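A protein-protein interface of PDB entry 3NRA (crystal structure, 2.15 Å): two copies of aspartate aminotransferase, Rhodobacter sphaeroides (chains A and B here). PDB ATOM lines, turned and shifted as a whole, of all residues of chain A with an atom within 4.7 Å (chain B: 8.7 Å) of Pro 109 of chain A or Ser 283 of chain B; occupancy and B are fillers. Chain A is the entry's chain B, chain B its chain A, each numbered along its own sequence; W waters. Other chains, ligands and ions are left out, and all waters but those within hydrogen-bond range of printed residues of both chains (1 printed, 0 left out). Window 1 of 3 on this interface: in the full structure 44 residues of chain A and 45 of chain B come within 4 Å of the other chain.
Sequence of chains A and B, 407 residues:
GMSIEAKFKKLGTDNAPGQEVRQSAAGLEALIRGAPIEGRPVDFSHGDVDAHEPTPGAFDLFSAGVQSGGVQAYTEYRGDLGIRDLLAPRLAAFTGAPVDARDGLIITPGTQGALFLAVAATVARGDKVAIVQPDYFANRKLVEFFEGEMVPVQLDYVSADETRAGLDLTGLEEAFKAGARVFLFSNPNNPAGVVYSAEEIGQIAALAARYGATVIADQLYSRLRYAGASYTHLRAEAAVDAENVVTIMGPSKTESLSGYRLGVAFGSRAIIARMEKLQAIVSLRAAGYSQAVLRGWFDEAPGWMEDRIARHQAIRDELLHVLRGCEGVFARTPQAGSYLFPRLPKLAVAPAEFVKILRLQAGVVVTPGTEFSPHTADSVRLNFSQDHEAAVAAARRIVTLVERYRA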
ATOM      1  N   THR A 108       0.857  20.534 -27.439  1.00  0.00           N
ATOM      2  CA  THR A 108       1.407  19.224 -27.055  1.00  0.00           C
ATOM      3  C   THR A 108       2.310  19.344 -25.805  1.00  0.00           C
ATOM      4  O   THR A 108       2.779  20.466 -25.466  1.00  0.00           O
ATOM      5  CB  THR A 108       2.289  18.640 -28.177  1.00  0.00           C
ATOM      6  OG1 THR A 108       3.309  19.580 -28.496  1.00  0.00           O
ATOM      7  CG2 THR A 108       1.472  18.320 -29.445  1.00  0.00           C
ATOM      8  N   PRO A 109       2.586  18.190 -25.129  1.00  0.00           N
ATOM      9  CA  PRO A 109       3.541  18.183 -24.012  1.00  0.00           C
ATOM     10  C   PRO A 109       4.995  18.312 -24.506  1.00  0.00           C
ATOM     11  O   PRO A 109       5.681  17.298 -24.751  1.00  0.00           O
ATOM     12  CB  PRO A 109       3.284  16.849 -23.320  1.00  0.00           C
ATOM     13  CG  PRO A 109       2.588  15.983 -24.375  1.00  0.00           C
ATOM     14  CD  PRO A 109       1.851  16.907 -25.255  1.00  0.00           C
ATOM     15  N   GLY A 110       5.439  19.564 -24.663  1.00  0.00           N
ATOM     16  CA  GLY A 110       6.740  19.855 -25.231  1.00  0.00           C
ATOM     17  C   GLY A 110       6.697  19.674 -26.735  1.00  0.00           C
ATOM     18  O   GLY A 110       5.702  19.152 -27.299  1.00  0.00           O
ATOM     19  N   THR A 111       7.730  20.157 -27.394  1.00  0.00           N
ATOM     20  CA  THR A 111       7.954  19.835 -28.782  1.00  0.00           C
ATOM     21  C   THR A 111       8.292  18.344 -28.919  1.00  0.00           C
ATOM     22  O   THR A 111       7.997  17.727 -29.970  1.00  0.00           O
ATOM     23  CB  THR A 111       9.062  20.727 -29.398  1.00  0.00           C
ATOM     24  OG1 THR A 111       8.620  22.065 -29.389  1.00  0.00           O
ATOM     25  CG2 THR A 111       9.357  20.354 -30.820  1.00  0.00           C
ATOM     26  N   GLN A 112       8.879  17.742 -27.866  1.00  0.00           N
ATOM     27  CA  GLN A 112       9.033  16.265 -27.847  1.00  0.00           C
ATOM     28  C   GLN A 112       7.672  15.588 -28.004  1.00  0.00           C
ATOM     29  O   GLN A 112       7.542  14.632 -28.764  1.00  0.00           O
ATOM     30  CB  GLN A 112       9.710  15.773 -26.547  1.00  0.00           C
ATOM     31  CG  GLN A 112      10.091  14.277 -26.558  1.00  0.00           C
ATOM     32  CD  GLN A 112      11.072  13.931 -27.694  1.00  0.00           C
ATOM     33  OE1 GLN A 112      12.071  14.624 -27.889  1.00  0.00           O
ATOM     34  NE2 GLN A 112      10.786  12.849 -28.428  1.00  0.00           N
ATOM     35  N   GLY A 113       6.670  16.091 -27.264  1.00  0.00           N
ATOM     36  CA  GLY A 113       5.291  15.603 -27.383  1.00  0.00           C
ATOM     37  C   GLY A 113       4.782  15.636 -28.818  1.00  0.00           C
ATOM     38  O   GLY A 113       4.232  14.647 -29.304  1.00  0.00           O
ATOM     39  N   ARG A 261       6.465  22.510 -20.044  1.00  0.00           N
ATOM     40  CA  ARG A 261       6.237  21.367 -20.953  1.00  0.00           C
ATOM     41  C   ARG A 261       5.167  21.661 -22.075  1.00  0.00           C
ATOM     42  O   ARG A 261       4.068  21.085 -22.077  1.00  0.00           O
ATOM     43  CB  ARG A 261       5.895  20.099 -20.161  1.00  0.00           C
ATOM     44  CG  ARG A 261       6.102  18.743 -20.973  1.00  0.00           C
ATOM     45  CD  ARG A 261       7.399  18.047 -20.567  1.00  0.00           C
ATOM     46  NE  ARG A 261       8.552  18.896 -20.791  1.00  0.00           N
ATOM     47  CZ  ARG A 261       9.221  19.015 -21.933  1.00  0.00           C
ATOM     48  NH1 ARG A 261       8.960  18.244 -22.978  1.00  0.00           N
ATOM     49  NH2 ARG A 261      10.188  19.905 -22.009  1.00  0.00           N
ATOM     50  N   LEU A 262       5.543  22.528 -23.034  1.00  0.00           N
ATOM     51  CA  LEU A 262       4.643  22.984 -24.079  1.00  0.00           C
ATOM     52  C   LEU A 262       5.302  22.938 -25.425  1.00  0.00           C
ATOM     53  O   LEU A 262       6.475  23.261 -25.558  1.00  0.00           O
ATOM     54  CB  LEU A 262       4.159  24.425 -23.797  1.00  0.00           C
ATOM     55  CG  LEU A 262       3.388  24.571 -22.497  1.00  0.00           C
ATOM     56  CD1 LEU A 262       3.422  26.005 -22.047  1.00  0.00           C
ATOM     57  CD2 LEU A 262       1.944  24.047 -22.673  1.00  0.00           C
ATOM     58  N   GLY A 263       4.551  22.469 -26.425  1.00  0.00           N
ATOM     59  CA  GLY A 263       4.968  22.538 -27.798  1.00  0.00           C
ATOM     60  C   GLY A 263       3.765  22.694 -28.648  1.00  0.00           C
ATOM     61  O   GLY A 263       2.633  22.578 -28.162  1.00  0.00           O
ATOM     62  N   GLN A 279      -3.167  11.792 -29.058  1.00  0.00           N
ATOM     63  CA  GLN A 279      -2.868  12.540 -27.811  1.00  0.00           C
ATOM     64  C   GLN A 279      -3.860  12.206 -26.685  1.00  0.00           C
ATOM     65  O   GLN A 279      -3.482  12.141 -25.511  1.00  0.00           O
ATOM     66  CB  GLN A 279      -2.858  14.064 -28.053  1.00  0.00           C
ATOM     67  CG  GLN A 279      -2.650  14.879 -26.768  1.00  0.00           C
ATOM     68  CD  GLN A 279      -1.840  16.149 -26.979  1.00  0.00           C
ATOM     69  OE1 GLN A 279      -0.609  16.117 -26.966  1.00  0.00           O
ATOM     70  NE2 GLN A 279      -2.530  17.277 -27.178  1.00  0.00           N
ATOM     71  N   SER A 283      -1.606  11.195 -23.316  1.00  0.00           N
ATOM     72  CA  SER A 283      -1.613  11.981 -22.060  1.00  0.00           C
ATOM     73  C   SER A 283      -2.816  12.936 -21.874  1.00  0.00           C
ATOM     74  O   SER A 283      -2.773  13.817 -20.985  1.00  0.00           O
ATOM     75  CB  SER A 283      -0.310  12.783 -21.953  1.00  0.00           C
ATOM     76  OG  SER A 283      -0.192  13.730 -23.018  1.00  0.00           O
ATOM     77  N   ALA A 286      -1.866  18.650 -23.317  1.00  0.00           N
ATOM     78  CA  ALA A 286      -0.847  19.459 -22.668  1.00  0.00           C
ATOM     79  C   ALA A 286      -1.445  19.997 -21.365  1.00  0.00           C
ATOM     80  O   ALA A 286      -2.613  20.398 -21.340  1.00  0.00           O
ATOM     81  CB  ALA A 286      -0.421  20.623 -23.597  1.00  0.00           C
ATOM     82  N   TYR B  77      14.193  11.726 -16.559  1.00  0.00           N
ATOM     83  CA  TYR B  77      13.017  11.390 -17.356  1.00  0.00           C
ATOM     84  C   TYR B  77      11.938  10.717 -16.479  1.00  0.00           C
ATOM     85  O   TYR B  77      10.765  11.010 -16.601  1.00  0.00           O
ATOM     86  CB  TYR B  77      13.391  10.459 -18.511  1.00  0.00           C
ATOM     87  CG  TYR B  77      14.385  11.019 -19.501  1.00  0.00           C
ATOM     88  CD1 TYR B  77      14.275  12.330 -19.971  1.00  0.00           C
ATOM     89  CD2 TYR B  77      15.386  10.218 -20.025  1.00  0.00           C
ATOM     90  CE1 TYR B  77      15.155  12.831 -20.903  1.00  0.00           C
ATOM     91  CE2 TYR B  77      16.292  10.710 -20.964  1.00  0.00           C
ATOM     92  CZ  TYR B  77      16.163  12.013 -21.415  1.00  0.00           C
ATOM     93  OH  TYR B  77      17.048  12.534 -22.344  1.00  0.00           O
ATOM     94  N   ILE B 107       7.199   9.115 -12.553  1.00  0.00           N
ATOM     95  CA  ILE B 107       6.241  10.191 -12.572  1.00  0.00           C
ATOM     96  C   ILE B 107       5.946  10.497 -14.028  1.00  0.00           C
ATOM     97  O   ILE B 107       6.872  10.622 -14.857  1.00  0.00           O
ATOM     98  CB  ILE B 107       6.772  11.452 -11.869  1.00  0.00           C
ATOM     99  CG1 ILE B 107       7.242  11.130 -10.462  1.00  0.00           C
ATOM    100  CG2 ILE B 107       5.681  12.519 -11.823  1.00  0.00           C
ATOM    101  CD1 ILE B 107       7.682  12.354  -9.671  1.00  0.00           C
ATOM    102  N   THR B 108       4.656  10.572 -14.355  1.00  0.00           N
ATOM    103  CA  THR B 108       4.181  10.603 -15.744  1.00  0.00           C
ATOM    104  C   THR B 108       3.265  11.808 -15.970  1.00  0.00           C
ATOM    105  O   THR B 108       2.776  12.389 -15.002  1.00  0.00           O
ATOM    106  CB  THR B 108       3.407   9.313 -16.049  1.00  0.00           C
ATOM    107  OG1 THR B 108       2.267   9.203 -15.168  1.00  0.00           O
ATOM    108  CG2 THR B 108       4.315   8.095 -15.844  1.00  0.00           C
ATOM    109  N   PRO B 109       2.989  12.163 -17.253  1.00  0.00           N
ATOM    110  CA  PRO B 109       1.998  13.199 -17.572  1.00  0.00           C
ATOM    111  C   PRO B 109       0.552  12.710 -17.396  1.00  0.00           C
ATOM    112  O   PRO B 109      -0.119  12.295 -18.370  1.00  0.00           O
ATOM    113  CB  PRO B 109       2.289  13.517 -19.048  1.00  0.00           C
ATOM    114  CG  PRO B 109       2.828  12.221 -19.591  1.00  0.00           C
ATOM    115  CD  PRO B 109       3.705  11.716 -18.475  1.00  0.00           C
ATOM    116  N   GLY B 110       0.080  12.794 -16.163  1.00  0.00           N
ATOM    117  CA  GLY B 110      -1.217  12.271 -15.791  1.00  0.00           C
ATOM    118  C   GLY B 110      -1.150  10.775 -15.587  1.00  0.00           C
ATOM    119  O   GLY B 110      -0.170  10.123 -15.982  1.00  0.00           O
ATOM    120  N   GLY B 113      -0.911   9.278 -18.973  1.00  0.00           N
ATOM    121  CA  GLY B 113       0.474   9.083 -19.358  1.00  0.00           C
ATOM    122  C   GLY B 113       1.070   7.768 -18.919  1.00  0.00           C
ATOM    123  O   GLY B 113       1.730   7.085 -19.712  1.00  0.00           O
ATOM    124  N   PHE B 116      -0.711   4.868 -20.920  1.00  0.00           N
ATOM    125  CA  PHE B 116      -0.096   4.727 -22.265  1.00  0.00           C
ATOM    126  C   PHE B 116       1.223   3.928 -22.222  1.00  0.00           C
ATOM    127  O   PHE B 116       1.435   2.981 -22.993  1.00  0.00           O
ATOM    128  CB  PHE B 116       0.181   6.110 -22.896  1.00  0.00           C
ATOM    129  CG  PHE B 116       0.762   6.022 -24.291  1.00  0.00           C
ATOM    130  CD1 PHE B 116      -0.024   5.644 -25.341  1.00  0.00           C
ATOM    131  CD2 PHE B 116       2.126   6.218 -24.516  1.00  0.00           C
ATOM    132  CE1 PHE B 116       0.508   5.516 -26.640  1.00  0.00           C
ATOM    133  CE2 PHE B 116       2.683   6.075 -25.804  1.00  0.00           C
ATOM    134  CZ  PHE B 116       1.865   5.733 -26.867  1.00  0.00           C
ATOM    135  N   LEU B 117       2.108   4.339 -21.331  1.00  0.00           N
ATOM    136  CA  LEU B 117       3.451   3.771 -21.247  1.00  0.00           C
ATOM    137  C   LEU B 117       3.396   2.333 -20.753  1.00  0.00           C
ATOM    138  O   LEU B 117       4.165   1.488 -21.224  1.00  0.00           O
ATOM    139  CB  LEU B 117       4.348   4.624 -20.315  1.00  0.00           C
ATOM    140  CG  LEU B 117       4.650   6.078 -20.733  1.00  0.00           C
ATOM    141  CD1 LEU B 117       5.216   6.867 -19.537  1.00  0.00           C
ATOM    142  CD2 LEU B 117       5.619   6.204 -21.963  1.00  0.00           C
ATOM    143  N   ARG B 261      -1.321  17.966 -14.579  1.00  0.00           N
ATOM    144  CA  ARG B 261      -1.017  16.792 -15.415  1.00  0.00           C
ATOM    145  C   ARG B 261       0.052  15.868 -14.813  1.00  0.00           C
ATOM    146  O   ARG B 261       1.167  15.730 -15.350  1.00  0.00           O
ATOM    147  CB  ARG B 261      -0.640  17.210 -16.845  1.00  0.00           C
ATOM    148  CG  ARG B 261      -0.762  16.070 -17.877  1.00  0.00           C
ATOM    149  CD  ARG B 261      -2.002  16.232 -18.772  1.00  0.00           C
ATOM    150  NE  ARG B 261      -3.198  16.193 -17.967  1.00  0.00           N
ATOM    151  CZ  ARG B 261      -3.818  15.089 -17.563  1.00  0.00           C
ATOM    152  NH1 ARG B 261      -3.442  13.877 -17.993  1.00  0.00           N
ATOM    153  NH2 ARG B 261      -4.841  15.200 -16.744  1.00  0.00           N
ATOM    154  N   MET B 275       9.144   1.690 -19.397  1.00  0.00           N
ATOM    155  CA  MET B 275       8.306   2.900 -19.366  1.00  0.00           C
ATOM    156  C   MET B 275       9.134   4.202 -19.325  1.00  0.00           C
ATOM    157  O   MET B 275       8.826   5.161 -20.044  1.00  0.00           O
ATOM    158  CB  MET B 275       7.351   2.851 -18.175  1.00  0.00           C
ATOM    159  CG  MET B 275       6.255   1.794 -18.287  1.00  0.00           C
ATOM    160  SD  MET B 275       5.220   1.619 -16.684  1.00  0.00           S
ATOM    161  CE  MET B 275       4.394   3.355 -16.684  1.00  0.00           C
ATOM    162  N   GLU B 276      10.187   4.212 -18.509  1.00  0.00           N
ATOM    163  CA  GLU B 276      11.076   5.367 -18.415  1.00  0.00           C
ATOM    164  C   GLU B 276      11.792   5.644 -19.752  1.00  0.00           C
ATOM    165  O   GLU B 276      11.956   6.824 -20.144  1.00  0.00           O
ATOM    166  CB  GLU B 276      12.097   5.174 -17.271  1.00  0.00           C
ATOM    167  CG  GLU B 276      11.449   5.277 -15.864  1.00  0.00           C
ATOM    168  CD  GLU B 276      12.282   4.646 -14.725  1.00  0.00           C
ATOM    169  OE1 GLU B 276      13.342   4.042 -14.981  1.00  0.00           O
ATOM    170  OE2 GLU B 276      11.849   4.761 -13.568  1.00  0.00           O
ATOM    171  N   LYS B 277      12.231   4.583 -20.433  1.00  0.00           N
ATOM    172  CA  LYS B 277      12.958   4.732 -21.697  1.00  0.00           C
ATOM    173  C   LYS B 277      12.039   5.279 -22.759  1.00  0.00           C
ATOM    174  O   LYS B 277      12.437   6.144 -23.529  1.00  0.00           O
ATOM    175  CB  LYS B 277      13.580   3.378 -22.167  1.00  0.00           C
ATOM    176  CG  LYS B 277      14.804   2.892 -21.338  1.00  0.00           C
ATOM    177  CD  LYS B 277      15.161   1.401 -21.676  1.00  0.00           C
ATOM    178  CE  LYS B 277      16.464   0.912 -20.987  1.00  0.00           C
ATOM    179  N   LEU B 278      10.801   4.772 -22.804  1.00  0.00           N
ATOM    180  CA  LEU B 278       9.806   5.264 -23.750  1.00  0.00           C
ATOM    181  C   LEU B 278       9.378   6.722 -23.454  1.00  0.00           C
ATOM    182  O   LEU B 278       9.184   7.507 -24.382  1.00  0.00           O
ATOM    183  CB  LEU B 278       8.583   4.365 -23.767  1.00  0.00           C
ATOM    184  CG  LEU B 278       7.432   4.763 -24.709  1.00  0.00           C
ATOM    185  CD1 LEU B 278       7.964   4.938 -26.143  1.00  0.00           C
ATOM    186  CD2 LEU B 278       6.291   3.717 -24.684  1.00  0.00           C
ATOM    187  N   GLN B 279       9.205   7.058 -22.177  1.00  0.00           N
ATOM    188  CA  GLN B 279       8.812   8.417 -21.783  1.00  0.00           C
ATOM    189  C   GLN B 279       9.776   9.450 -22.347  1.00  0.00           C
ATOM    190  O   GLN B 279       9.355  10.531 -22.714  1.00  0.00           O
ATOM    191  CB  GLN B 279       8.733   8.564 -20.244  1.00  0.00           C
ATOM    192  CG  GLN B 279       8.504  10.012 -19.753  1.00  0.00           C
ATOM    193  CD  GLN B 279       7.589  10.097 -18.553  1.00  0.00           C
ATOM    194  OE1 GLN B 279       6.356  10.041 -18.694  1.00  0.00           O
ATOM    195  NE2 GLN B 279       8.185  10.252 -17.339  1.00  0.00           N
ATOM    196  N   ALA B 280      11.074   9.106 -22.409  1.00  0.00           N
ATOM    197  CA  ALA B 280      12.081  10.025 -22.920  1.00  0.00           C
ATOM    198  C   ALA B 280      11.733  10.543 -24.323  1.00  0.00           C
ATOM    199  O   ALA B 280      11.976  11.730 -24.631  1.00  0.00           O
ATOM    200  CB  ALA B 280      13.472   9.355 -22.931  1.00  0.00           C
ATOM    201  N   ILE B 281      11.173   9.661 -25.161  1.00  0.00           N
ATOM    202  CA  ILE B 281      10.784  10.023 -26.528  1.00  0.00           C
ATOM    203  C   ILE B 281       9.282  10.366 -26.734  1.00  0.00           C
ATOM    204  O   ILE B 281       8.941  10.951 -27.758  1.00  0.00           O
ATOM    205  CB  ILE B 281      11.285   8.967 -27.571  1.00  0.00           C
ATOM    206  CG1 ILE B 281      10.534   7.636 -27.476  1.00  0.00           C
ATOM    207  CG2 ILE B 281      12.733   8.718 -27.379  1.00  0.00           C
ATOM    208  CD1 ILE B 281      11.020   6.634 -28.506  1.00  0.00           C
ATOM    209  N   VAL B 282       8.414  10.069 -25.739  1.00  0.00           N
ATOM    210  CA  VAL B 282       7.007  10.473 -25.780  1.00  0.00           C
ATOM    211  C   VAL B 282       6.833  11.937 -25.385  1.00  0.00           C
ATOM    212  O   VAL B 282       6.088  12.669 -26.017  1.00  0.00           O
ATOM    213  CB  VAL B 282       6.143   9.598 -24.863  1.00  0.00           C
ATOM    214  CG1 VAL B 282       4.714  10.129 -24.797  1.00  0.00           C
ATOM    215  CG2 VAL B 282       6.142   8.113 -25.352  1.00  0.00           C
ATOM    216  N   SER B 283       7.484  12.357 -24.313  1.00  0.00           N
ATOM    217  CA  SER B 283       7.339  13.744 -23.828  1.00  0.00           C
ATOM    218  C   SER B 283       8.486  14.257 -22.953  1.00  0.00           C
ATOM    219  O   SER B 283       8.355  15.353 -22.371  1.00  0.00           O
ATOM    220  CB  SER B 283       6.012  13.892 -23.050  1.00  0.00           C
ATOM    221  OG  SER B 283       6.032  13.157 -21.837  1.00  0.00           O
ATOM    222  N   LEU B 284       9.627  13.509 -22.932  1.00  0.00           N
ATOM    223  CA  LEU B 284      10.781  13.703 -22.012  1.00  0.00           C
ATOM    224  C   LEU B 284      10.468  13.356 -20.553  1.00  0.00           C
ATOM    225  O   LEU B 284      11.074  12.447 -20.009  1.00  0.00           O
ATOM    226  CB  LEU B 284      11.391  15.109 -22.100  1.00  0.00           C
ATOM    227  CG  LEU B 284      11.877  15.650 -23.452  1.00  0.00           C
ATOM    228  CD1 LEU B 284      12.334  17.142 -23.287  1.00  0.00           C
ATOM    229  CD2 LEU B 284      12.989  14.812 -24.041  1.00  0.00           C
ATOM    230  N   ARG B 285       9.518  14.079 -19.937  1.00  0.00           N
ATOM    231  CA  ARG B 285       9.250  13.989 -18.498  1.00  0.00           C
ATOM    232  C   ARG B 285       7.871  14.585 -18.194  1.00  0.00           C
ATOM    233  O   ARG B 285       7.366  15.370 -18.971  1.00  0.00           O
ATOM    234  CB  ARG B 285      10.322  14.779 -17.707  1.00  0.00           C
ATOM    235  CG  ARG B 285      10.420  16.317 -18.076  1.00  0.00           C
ATOM    236  CD  ARG B 285      11.482  17.026 -17.280  1.00  0.00           C
ATOM    237  NE  ARG B 285      12.786  16.428 -17.554  1.00  0.00           N
ATOM    238  CZ  ARG B 285      13.565  16.717 -18.601  1.00  0.00           C
ATOM    239  NH1 ARG B 285      13.246  17.689 -19.460  1.00  0.00           N
ATOM    240  NH2 ARG B 285      14.682  16.012 -18.794  1.00  0.00           N
ATOM    241  N   ALA B 286       7.291  14.250 -17.044  1.00  0.00           N
ATOM    242  CA  ALA B 286       6.204  15.077 -16.483  1.00  0.00           C
ATOM    243  C   ALA B 286       6.711  16.493 -16.311  1.00  0.00           C
ATOM    244  O   ALA B 286       7.869  16.701 -15.997  1.00  0.00           O
ATOM    245  CB  ALA B 286       5.728  14.528 -15.152  1.00  0.00           C
ATOM    246  N   ALA B 287       5.856  17.467 -16.539  1.00  0.00           N
ATOM    247  CA  ALA B 287       6.297  18.843 -16.565  1.00  0.00           C
ATOM    248  C   ALA B 287       7.079  19.129 -15.286  1.00  0.00           C
ATOM    249  O   ALA B 287       6.602  18.873 -14.188  1.00  0.00           O
ATOM    250  CB  ALA B 287       5.101  19.794 -16.686  1.00  0.00           C
ATOM    251  N   GLY B 288       8.283  19.631 -15.440  1.00  0.00           N
ATOM    252  CA  GLY B 288       9.161  19.810 -14.327  1.00  0.00           C
ATOM    253  C   GLY B 288       8.541  20.644 -13.220  1.00  0.00           C
ATOM    254  O   GLY B 288       8.581  20.251 -12.064  1.00  0.00           O
HETATM  255  O   HOH W   1       3.118  13.041 -26.938  1.00  0.00           O
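Ser 283 of chain B touches Pro 109 of chain A (CB to O, 3.8 Å).
O of Ala 280 of chain B touches CG of Gln 112 of chain A, 3.7 Å away.
Val 282 of chain B touches Gln 112 of chain A (O to O, 3.7 Å).
CG of Gln 112 of chain A touches CA of Ser 283 of chain B, 3.9 Å away.
Leu 284 of chain B touches Gln 112 of chain A (N to CG, 3.7 Å).
CA of Gly 113 of chain A touches O of Val 282 of chain B, 3.3 Å away.
NH1 of Arg 261 of chain A touches CD1 of Leu 284 of chain B, 3.6 Å away.
Arg 285 of chain B touches Arg 261 of chain A.
Arg 261 of chain A touches Ala 287 of chain B (CB to CB, 3.6 Å).
Ser 283 of chain A touches Pro 109 of chain B (CB to O, 3.6 Å).
Pro 109 of chain A touches Ser 283 of chain B, and with the chains exchanged Ser 283 of chain A touches Pro 109 of chain B.
Arg 261 of chain A touches Ser 283 of chain B, and with the chains exchanged Ser 283 of chain A touches Arg 261 of chain B.
Hydrophobic or aromatic side chains of chain B within 4 Å of the printed part of chain A: Pro 109, Leu 284 and Ala 287.
Along chain B the printed residues that touch a printed residue of chain A span positions 109 to 287.
Among the printed residues, no Asp or Glu carboxylate lies within 4 Å of a Lys or Arg side-chain nitrogen of the other chain.
O of Ser 283 of chain A sits at hydrogen-bond distance from NH1 of Arg 261 of chain B (3.1 Å).
The side-chain amide nitrogen of Gln 112 of chain A sits at hydrogen-bond distance from the backbone carbonyl oxygen of Ile 281 of chain B (2.7 Å).
The backbone carbonyl oxygen (O) of Ser 283 of chain B lies within hydrogen-bond range of the guanidinium group (NH1) of Arg 261 of chain A, at 3.0 Å.
Water W1 bridges the backbone carbonyl oxygen of Gly 113 of chain A (3.1 Å) and the backbone carbonyl oxygen of Val 282 of chain B (3.1 Å).
N of Gly 110 of chain B sits at hydrogen-bond distance from O of Arg 261 of chain B.
The backbone carbonyl oxygen (O) of Gln 279 of chain B lies within hydrogen-bond range of the backbone NH (N) of Leu 284 of chain B, at 3.0 Å.
N of Gly 110 of chain A is in hydrogen-bond range of O of Arg 261 of chain A (3.3 Å).
Of chain B, only Ser 283 comes within 4 Å of Pro 109 of chain A.
Ser 283 of chain B touches just these residues of chain A: Pro 109, Gln 112 and Arg 261.
Thr 108 of chain A touches none of the printed residues of chain B.
No residue of chain B comes within 4 Å of Gly 110 of chain A.
Printed residues of chain B within 4 Å of Gln 112 of chain A: Ala 280, Ile 281, Val 282, Ser 283 and Leu 284.
Of the printed residues of chain A, Pro 109 of chain B touches Ser 283 (3.6 Å).
Printed residues of chain A within 4 Å of Arg 261 of chain B: Ser 283 (3.1 Å).
Printed residues of chain B within 4 Å of Ser 283 of chain A: Pro 109 (3.6 Å) and Arg 261 (3.1 Å).
Of the printed residues of chain A, Ile 281 of chain B touches Gln 112.
The nearest residue of chain B that does not touch Pro 109 of chain A is Val 282 of chain B (4.8 Å).
The nearest printed residue of chain B that does not touch Arg 261 of chain A is Ala 286 of chain B (4.6 Å).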
